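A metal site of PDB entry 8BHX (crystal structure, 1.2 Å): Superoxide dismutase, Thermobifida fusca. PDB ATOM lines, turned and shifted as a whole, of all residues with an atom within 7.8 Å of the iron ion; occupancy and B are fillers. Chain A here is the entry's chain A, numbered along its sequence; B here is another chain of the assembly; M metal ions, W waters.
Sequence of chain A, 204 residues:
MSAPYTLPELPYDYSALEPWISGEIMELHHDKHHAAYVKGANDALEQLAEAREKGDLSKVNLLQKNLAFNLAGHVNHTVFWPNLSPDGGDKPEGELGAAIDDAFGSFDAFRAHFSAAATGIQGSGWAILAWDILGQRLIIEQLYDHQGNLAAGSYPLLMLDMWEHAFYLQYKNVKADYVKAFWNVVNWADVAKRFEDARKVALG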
ATOM      1  N   HIS A  29      19.651 -21.791  14.569  1.00  0.00           N
ATOM      2  CA  HIS A  29      18.394 -21.517  13.899  1.00  0.00           C
ATOM      3  C   HIS A  29      18.491 -21.789  12.406  1.00  0.00           C
ATOM      4  O   HIS A  29      17.625 -22.466  11.820  1.00  0.00           O
ATOM      5  CB  HIS A  29      18.012 -20.065  14.186  1.00  0.00           C
ATOM      6  CG  HIS A  29      16.589 -19.765  13.867  1.00  0.00           C
ATOM      7  ND1 HIS A  29      16.080 -18.485  13.924  1.00  0.00           N
ATOM      8  CD2 HIS A  29      15.546 -20.565  13.519  1.00  0.00           C
ATOM      9  CE1 HIS A  29      14.791 -18.512  13.629  1.00  0.00           C
ATOM     10  NE2 HIS A  29      14.441 -19.761  13.374  1.00  0.00           N
ATOM     11  N   HIS A  30      19.538 -21.289  11.765  1.00  0.00           N
ATOM     12  CA  HIS A  30      19.699 -21.494  10.333  1.00  0.00           C
ATOM     13  C   HIS A  30      20.231 -22.889  10.015  1.00  0.00           C
ATOM     14  O   HIS A  30      19.665 -23.603   9.170  1.00  0.00           O
ATOM     15  CB  HIS A  30      20.640 -20.429   9.766  1.00  0.00           C
ATOM     16  CG  HIS A  30      21.039 -20.667   8.345  1.00  0.00           C
ATOM     17  ND1 HIS A  30      22.083 -21.483   7.989  1.00  0.00           N
ATOM     18  CD2 HIS A  30      20.489 -20.222   7.192  1.00  0.00           C
ATOM     19  CE1 HIS A  30      22.177 -21.516   6.666  1.00  0.00           C
ATOM     20  NE2 HIS A  30      21.220 -20.772   6.168  1.00  0.00           N
ATOM     21  N   HIS A  33      17.640 -25.740  12.362  1.00  0.00           N
ATOM     22  CA  HIS A  33      16.186 -25.701  12.211  1.00  0.00           C
ATOM     23  C   HIS A  33      15.774 -25.533  10.749  1.00  0.00           C
ATOM     24  O   HIS A  33      14.910 -26.250  10.238  1.00  0.00           O
ATOM     25  CB  HIS A  33      15.529 -24.620  13.079  1.00  0.00           C
ATOM     26  CG  HIS A  33      15.615 -24.875  14.550  1.00  0.00           C
ATOM     27  ND1 HIS A  33      14.628 -25.511  15.257  1.00  0.00           N
ATOM     28  CD2 HIS A  33      16.568 -24.539  15.448  1.00  0.00           C
ATOM     29  CE1 HIS A  33      14.969 -25.574  16.533  1.00  0.00           C
ATOM     30  NE2 HIS A  33      16.141 -24.994  16.674  1.00  0.00           N
ATOM     31  N   HIS A  34      16.360 -24.556  10.046  1.00  0.00           N
ATOM     32  CA  HIS A  34      15.943 -24.363   8.657  1.00  0.00           C
ATOM     33  C   HIS A  34      16.313 -25.565   7.806  1.00  0.00           C
ATOM     34  O   HIS A  34      15.504 -26.043   6.991  1.00  0.00           O
ATOM     35  CB  HIS A  34      16.505 -23.053   8.108  1.00  0.00           C
ATOM     36  CG  HIS A  34      15.895 -22.613   6.810  1.00  0.00           C
ATOM     37  ND1 HIS A  34      16.233 -21.430   6.190  1.00  0.00           N
ATOM     38  CD2 HIS A  34      14.979 -23.215   6.005  1.00  0.00           C
ATOM     39  CE1 HIS A  34      15.545 -21.314   5.066  1.00  0.00           C
ATOM     40  NE2 HIS A  34      14.772 -22.368   4.930  1.00  0.00           N
ATOM     41  N   TYR A  37      13.525 -28.125   7.803  1.00  0.00           N
ATOM     42  CA  TYR A  37      12.359 -27.856   6.960  1.00  0.00           C
ATOM     43  C   TYR A  37      12.651 -28.153   5.502  1.00  0.00           C
ATOM     44  O   TYR A  37      11.773 -28.647   4.784  1.00  0.00           O
ATOM     45  CB  TYR A  37      11.878 -26.408   7.110  1.00  0.00           C
ATOM     46  CG  TYR A  37      11.564 -26.009   8.509  1.00  0.00           C
ATOM     47  CD1 TYR A  37      12.150 -24.878   9.064  1.00  0.00           C
ATOM     48  CD2 TYR A  37      10.696 -26.755   9.296  1.00  0.00           C
ATOM     49  CE1 TYR A  37      11.874 -24.505  10.354  1.00  0.00           C
ATOM     50  CE2 TYR A  37      10.423 -26.369  10.606  1.00  0.00           C
ATOM     51  CZ  TYR A  37      11.029 -25.251  11.113  1.00  0.00           C
ATOM     52  OH  TYR A  37      10.727 -24.879  12.416  1.00  0.00           O
ATOM     53  N   GLY A  73       7.581 -23.599   6.674  1.00  0.00           N
ATOM     54  CA  GLY A  73       8.774 -23.270   7.441  1.00  0.00           C
ATOM     55  C   GLY A  73       9.911 -22.818   6.541  1.00  0.00           C
ATOM     56  O   GLY A  73      10.620 -21.862   6.851  1.00  0.00           O
ATOM     57  N   ASN A  76       9.053 -19.318   5.132  1.00  0.00           N
ATOM     58  CA  ASN A  76       9.094 -18.274   6.134  1.00  0.00           C
ATOM     59  C   ASN A  76      10.537 -17.918   6.491  1.00  0.00           C
ATOM     60  O   ASN A  76      10.884 -16.733   6.612  1.00  0.00           O
ATOM     61  CB  ASN A  76       8.346 -18.714   7.392  1.00  0.00           C
ATOM     62  CG  ASN A  76       6.846 -18.871   7.197  1.00  0.00           C
ATOM     63  OD1 ASN A  76       6.298 -18.491   6.178  1.00  0.00           O
ATOM     64  ND2 ASN A  76       6.188 -19.430   8.193  1.00  0.00           N
ATOM     65  N   HIS A  77      11.402 -18.924   6.662  1.00  0.00           N
ATOM     66  CA  HIS A  77      12.779 -18.635   7.017  1.00  0.00           C
ATOM     67  C   HIS A  77      13.568 -18.094   5.831  1.00  0.00           C
ATOM     68  O   HIS A  77      14.488 -17.287   6.004  1.00  0.00           O
ATOM     69  CB  HIS A  77      13.474 -19.876   7.619  1.00  0.00           C
ATOM     70  CG  HIS A  77      12.940 -20.262   8.976  1.00  0.00           C
ATOM     71  ND1 HIS A  77      11.818 -21.034   9.133  1.00  0.00           N
ATOM     72  CD2 HIS A  77      13.370 -19.960  10.226  1.00  0.00           C
ATOM     73  CE1 HIS A  77      11.570 -21.205  10.417  1.00  0.00           C
ATOM     74  NE2 HIS A  77      12.497 -20.556  11.107  1.00  0.00           N
ATOM     75  N   PHE A  80      12.886 -14.597   6.105  1.00  0.00           N
ATOM     76  CA  PHE A  80      13.383 -14.041   7.353  1.00  0.00           C
ATOM     77  C   PHE A  80      14.860 -13.613   7.269  1.00  0.00           C
ATOM     78  O   PHE A  80      15.203 -12.501   7.686  1.00  0.00           O
ATOM     79  CB  PHE A  80      13.172 -15.075   8.480  1.00  0.00           C
ATOM     80  CG  PHE A  80      13.481 -14.578   9.878  1.00  0.00           C
ATOM     81  CD1 PHE A  80      12.884 -13.414  10.393  1.00  0.00           C
ATOM     82  CD2 PHE A  80      14.288 -15.322  10.718  1.00  0.00           C
ATOM     83  CE1 PHE A  80      13.157 -12.996  11.709  1.00  0.00           C
ATOM     84  CE2 PHE A  80      14.578 -14.900  12.030  1.00  0.00           C
ATOM     85  CZ  PHE A  80      13.978 -13.762  12.517  1.00  0.00           C
ATOM     86  N   TRP A  81      15.752 -14.467   6.762  1.00  0.00           N
ATOM     87  CA  TRP A  81      17.172 -14.114   6.856  1.00  0.00           C
ATOM     88  C   TRP A  81      17.501 -12.796   6.151  1.00  0.00           C
ATOM     89  O   TRP A  81      18.157 -11.951   6.778  1.00  0.00           O
ATOM     90  CB  TRP A  81      18.128 -15.243   6.400  1.00  0.00           C
ATOM     91  CG  TRP A  81      17.793 -16.618   6.913  1.00  0.00           C
ATOM     92  CD1 TRP A  81      17.553 -17.706   6.150  1.00  0.00           C
ATOM     93  CD2 TRP A  81      17.638 -17.040   8.283  1.00  0.00           C
ATOM     94  NE1 TRP A  81      17.262 -18.788   6.941  1.00  0.00           N
ATOM     95  CE2 TRP A  81      17.324 -18.409   8.252  1.00  0.00           C
ATOM     96  CE3 TRP A  81      17.773 -16.403   9.526  1.00  0.00           C
ATOM     97  CZ2 TRP A  81      17.095 -19.151   9.403  1.00  0.00           C
ATOM     98  CZ3 TRP A  81      17.561 -17.142  10.673  1.00  0.00           C
ATOM     99  CH2 TRP A  81      17.220 -18.504  10.611  1.00  0.00           C
ATOM    100  N   GLY A 125       4.646 -19.262  16.354  1.00  0.00           N
ATOM    101  CA  GLY A 125       4.088 -18.532  15.238  1.00  0.00           C
ATOM    102  C   GLY A 125       4.985 -17.390  14.793  1.00  0.00           C
ATOM    103  O   GLY A 125       6.169 -17.324  15.156  1.00  0.00           O
ATOM    104  N   TRP A 126       4.398 -16.504  13.996  1.00  0.00           N
ATOM    105  CA  TRP A 126       5.087 -15.383  13.376  1.00  0.00           C
ATOM    106  C   TRP A 126       4.190 -14.153  13.369  1.00  0.00           C
ATOM    107  O   TRP A 126       2.965 -14.273  13.310  1.00  0.00           O
ATOM    108  CB  TRP A 126       5.414 -15.640  11.893  1.00  0.00           C
ATOM    109  CG  TRP A 126       6.244 -16.861  11.640  1.00  0.00           C
ATOM    110  CD1 TRP A 126       5.866 -18.169  11.788  1.00  0.00           C
ATOM    111  CD2 TRP A 126       7.607 -16.882  11.200  1.00  0.00           C
ATOM    112  NE1 TRP A 126       6.923 -18.995  11.480  1.00  0.00           N
ATOM    113  CE2 TRP A 126       7.993 -18.222  11.110  1.00  0.00           C
ATOM    114  CE3 TRP A 126       8.526 -15.893  10.847  1.00  0.00           C
ATOM    115  CZ2 TRP A 126       9.265 -18.613  10.705  1.00  0.00           C
ATOM    116  CZ3 TRP A 126       9.781 -16.270  10.431  1.00  0.00           C
ATOM    117  CH2 TRP A 126      10.147 -17.623  10.375  1.00  0.00           C
ATOM    118  N   HIS A 146       3.840 -22.502  11.281  1.00  0.00           N
ATOM    119  CA  HIS A 146       4.295 -21.863  10.060  1.00  0.00           C
ATOM    120  C   HIS A 146       3.195 -21.596   9.047  1.00  0.00           C
ATOM    121  O   HIS A 146       3.359 -20.718   8.202  1.00  0.00           O
ATOM    122  CB  HIS A 146       5.352 -22.730   9.354  1.00  0.00           C
ATOM    123  CG  HIS A 146       6.585 -22.924  10.156  1.00  0.00           C
ATOM    124  ND1 HIS A 146       7.244 -21.871  10.756  1.00  0.00           N
ATOM    125  CD2 HIS A 146       7.268 -24.042  10.485  1.00  0.00           C
ATOM    126  CE1 HIS A 146       8.301 -22.341  11.397  1.00  0.00           C
ATOM    127  NE2 HIS A 146       8.321 -23.656  11.268  1.00  0.00           N
ATOM    128  N   ASP A 161      10.026 -14.186  13.423  1.00  0.00           N
ATOM    129  CA  ASP A 161       9.846 -15.535  13.948  1.00  0.00           C
ATOM    130  C   ASP A 161       9.676 -15.469  15.455  1.00  0.00           C
ATOM    131  O   ASP A 161      10.580 -15.032  16.162  1.00  0.00           O
ATOM    132  CB  ASP A 161      11.096 -16.333  13.608  1.00  0.00           C
ATOM    133  CG  ASP A 161      10.970 -17.808  13.865  1.00  0.00           C
ATOM    134  OD1 ASP A 161       9.954 -18.273  14.417  1.00  0.00           O
ATOM    135  OD2 ASP A 161      11.947 -18.512  13.548  1.00  0.00           O
ATOM    136  N   MET A 162       8.513 -15.913  15.939  1.00  0.00           N
ATOM    137  CA  MET A 162       8.197 -15.933  17.355  1.00  0.00           C
ATOM    138  C   MET A 162       8.160 -17.334  17.929  1.00  0.00           C
ATOM    139  O   MET A 162       7.680 -17.521  19.044  1.00  0.00           O
ATOM    140  CB  MET A 162       6.889 -15.172  17.653  1.00  0.00           C
ATOM    141  CG  MET A 162       6.976 -13.701  17.281  1.00  0.00           C
ATOM    142  SD  MET A 162       8.222 -12.773  18.199  1.00  0.00           S
ATOM    143  CE  MET A 162       7.740 -13.084  19.896  1.00  0.00           C
ATOM    144  N   TRP A 163       8.679 -18.324  17.205  1.00  0.00           N
ATOM    145  CA  TRP A 163       8.949 -19.599  17.845  1.00  0.00           C
ATOM    146  C   TRP A 163       9.987 -19.387  18.947  1.00  0.00           C
ATOM    147  O   TRP A 163      10.890 -18.557  18.825  1.00  0.00           O
ATOM    148  CB  TRP A 163       9.509 -20.597  16.843  1.00  0.00           C
ATOM    149  CG  TRP A 163       8.498 -21.152  15.884  1.00  0.00           C
ATOM    150  CD1 TRP A 163       7.651 -20.465  15.058  1.00  0.00           C
ATOM    151  CD2 TRP A 163       8.276 -22.543  15.621  1.00  0.00           C
ATOM    152  NE1 TRP A 163       6.900 -21.354  14.310  1.00  0.00           N
ATOM    153  CE2 TRP A 163       7.268 -22.632  14.636  1.00  0.00           C
ATOM    154  CE3 TRP A 163       8.818 -23.710  16.147  1.00  0.00           C
ATOM    155  CZ2 TRP A 163       6.803 -23.855  14.159  1.00  0.00           C
ATOM    156  CZ3 TRP A 163       8.349 -24.922  15.663  1.00  0.00           C
ATOM    157  CH2 TRP A 163       7.360 -24.978  14.679  1.00  0.00           C
ATOM    158  N   GLU A 164       9.853 -20.149  20.026  1.00  0.00           N
ATOM    159  CA  GLU A 164      10.756 -19.962  21.148  1.00  0.00           C
ATOM    160  C   GLU A 164      12.211 -20.202  20.764  1.00  0.00           C
ATOM    161  O   GLU A 164      13.090 -19.531  21.303  1.00  0.00           O
ATOM    162  CB  GLU A 164      10.304 -20.833  22.323  1.00  0.00           C
ATOM    163  CG  GLU A 164       8.987 -20.370  22.945  1.00  0.00           C
ATOM    164  CD  GLU A 164       8.466 -21.255  24.050  1.00  0.00           C
ATOM    165  OE1 GLU A 164       8.506 -22.504  23.906  1.00  0.00           O
ATOM    166  OE2 GLU A 164       7.988 -20.707  25.072  1.00  0.00           O
ATOM    167  N   HIS A 165      12.508 -21.086  19.810  1.00  0.00           N
ATOM    168  CA  HIS A 165      13.897 -21.276  19.418  1.00  0.00           C
ATOM    169  C   HIS A 165      14.515 -20.006  18.843  1.00  0.00           C
ATOM    170  O   HIS A 165      15.748 -19.902  18.799  1.00  0.00           O
ATOM    171  CB  HIS A 165      14.061 -22.431  18.431  1.00  0.00           C
ATOM    172  CG  HIS A 165      13.366 -22.228  17.100  1.00  0.00           C
ATOM    173  ND1 HIS A 165      12.407 -23.096  16.649  1.00  0.00           N
ATOM    174  CD2 HIS A 165      13.538 -21.304  16.127  1.00  0.00           C
ATOM    175  CE1 HIS A 165      12.006 -22.719  15.442  1.00  0.00           C
ATOM    176  NE2 HIS A 165      12.670 -21.633  15.107  1.00  0.00           N
ATOM    177  N   ALA A 166      13.700 -19.055  18.395  1.00  0.00           N
ATOM    178  CA  ALA A 166      14.247 -17.849  17.783  1.00  0.00           C
ATOM    179  C   ALA A 166      14.793 -16.874  18.814  1.00  0.00           C
ATOM    180  O   ALA A 166      15.549 -15.962  18.453  1.00  0.00           O
ATOM    181  CB  ALA A 166      13.186 -17.145  16.934  1.00  0.00           C
ATOM    182  N   TYR A 178      12.918  -9.304  22.923  1.00  0.00           N
ATOM    183  CA  TYR A 178      13.305  -9.772  21.598  1.00  0.00           C
ATOM    184  C   TYR A 178      12.651  -8.931  20.521  1.00  0.00           C
ATOM    185  O   TYR A 178      13.301  -8.540  19.536  1.00  0.00           O
ATOM    186  CB  TYR A 178      12.930 -11.241  21.463  1.00  0.00           C
ATOM    187  CG  TYR A 178      12.970 -11.846  20.075  1.00  0.00           C
ATOM    188  CD1 TYR A 178      14.144 -11.931  19.335  1.00  0.00           C
ATOM    189  CD2 TYR A 178      11.827 -12.380  19.525  1.00  0.00           C
ATOM    190  CE1 TYR A 178      14.157 -12.519  18.091  1.00  0.00           C
ATOM    191  CE2 TYR A 178      11.837 -12.985  18.283  1.00  0.00           C
ATOM    192  CZ  TYR A 178      12.997 -13.060  17.567  1.00  0.00           C
ATOM    193  OH  TYR A 178      13.054 -13.661  16.320  1.00  0.00           O
ATOM    194  N   GLU B 164       9.277 -25.764  23.220  1.00  0.00           N
ATOM    195  CA  GLU B 164      10.721 -25.540  23.213  1.00  0.00           C
ATOM    196  C   GLU B 164      11.223 -24.978  24.540  1.00  0.00           C
ATOM    197  O   GLU B 164      12.338 -25.320  24.949  1.00  0.00           O
ATOM    198  CB  GLU B 164      11.107 -24.674  22.010  1.00  0.00           C
ATOM    199  CG  GLU B 164      10.889 -25.390  20.668  1.00  0.00           C
ATOM    200  CD  GLU B 164      11.206 -24.545  19.439  1.00  0.00           C
ATOM    201  OE1 GLU B 164      10.805 -23.358  19.425  1.00  0.00           O
ATOM    202  OE2 GLU B 164      11.844 -25.107  18.518  1.00  0.00           O
HETATM  203 FE    FE M   1      12.401 -20.477  13.265  1.00  0.00          FE
HETATM  204  O   HOH W   1      10.390 -20.891  13.301  1.00  0.00           O
HETATM  205  O   HOH W   2      12.832 -22.558  12.704  1.00  0.00           O
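The backbone carbonyl oxygen (O) of Asp 161 is in hydrogen-bond range of the side-chain hydroxyl (OH) of Tyr 178 (2.8 Å).
N of His 34 is in hydrogen-bond range of O of His 29 (3.0 Å).
NE1 of Trp 81 lies close to O of His 77.
The side-chain carboxylate (OE2) of Glu 164 of chain B sits at hydrogen-bond distance from a ring nitrogen (ND1) of His 165 (2.8 Å).
ND1 of His 77 lies within hydrogen-bond range of O of Gly 73 (2.7 Å).
The backbone NH (N) of Trp 163 sits at hydrogen-bond distance from the side-chain carboxylate (OD1) of Asp 161 (3.1 Å).
Four residues have an atom within 4 Å of the iron ion: His 29, His 77, Asp 161 and His 165.
The iron ion is bound by OD2 of Asp 161, 2.0 Å away.
Water W1 is bound to the iron ion (2.1 Å).
The iron ion is bound by a ring nitrogen (NE2) of His 77 (2.2 Å).
The iron ion is bound by NE2 of His 29, 2.2 Å away.
NE2 of His 165 binds the iron ion (2.2 Å).
Water W2 binds the iron ion.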
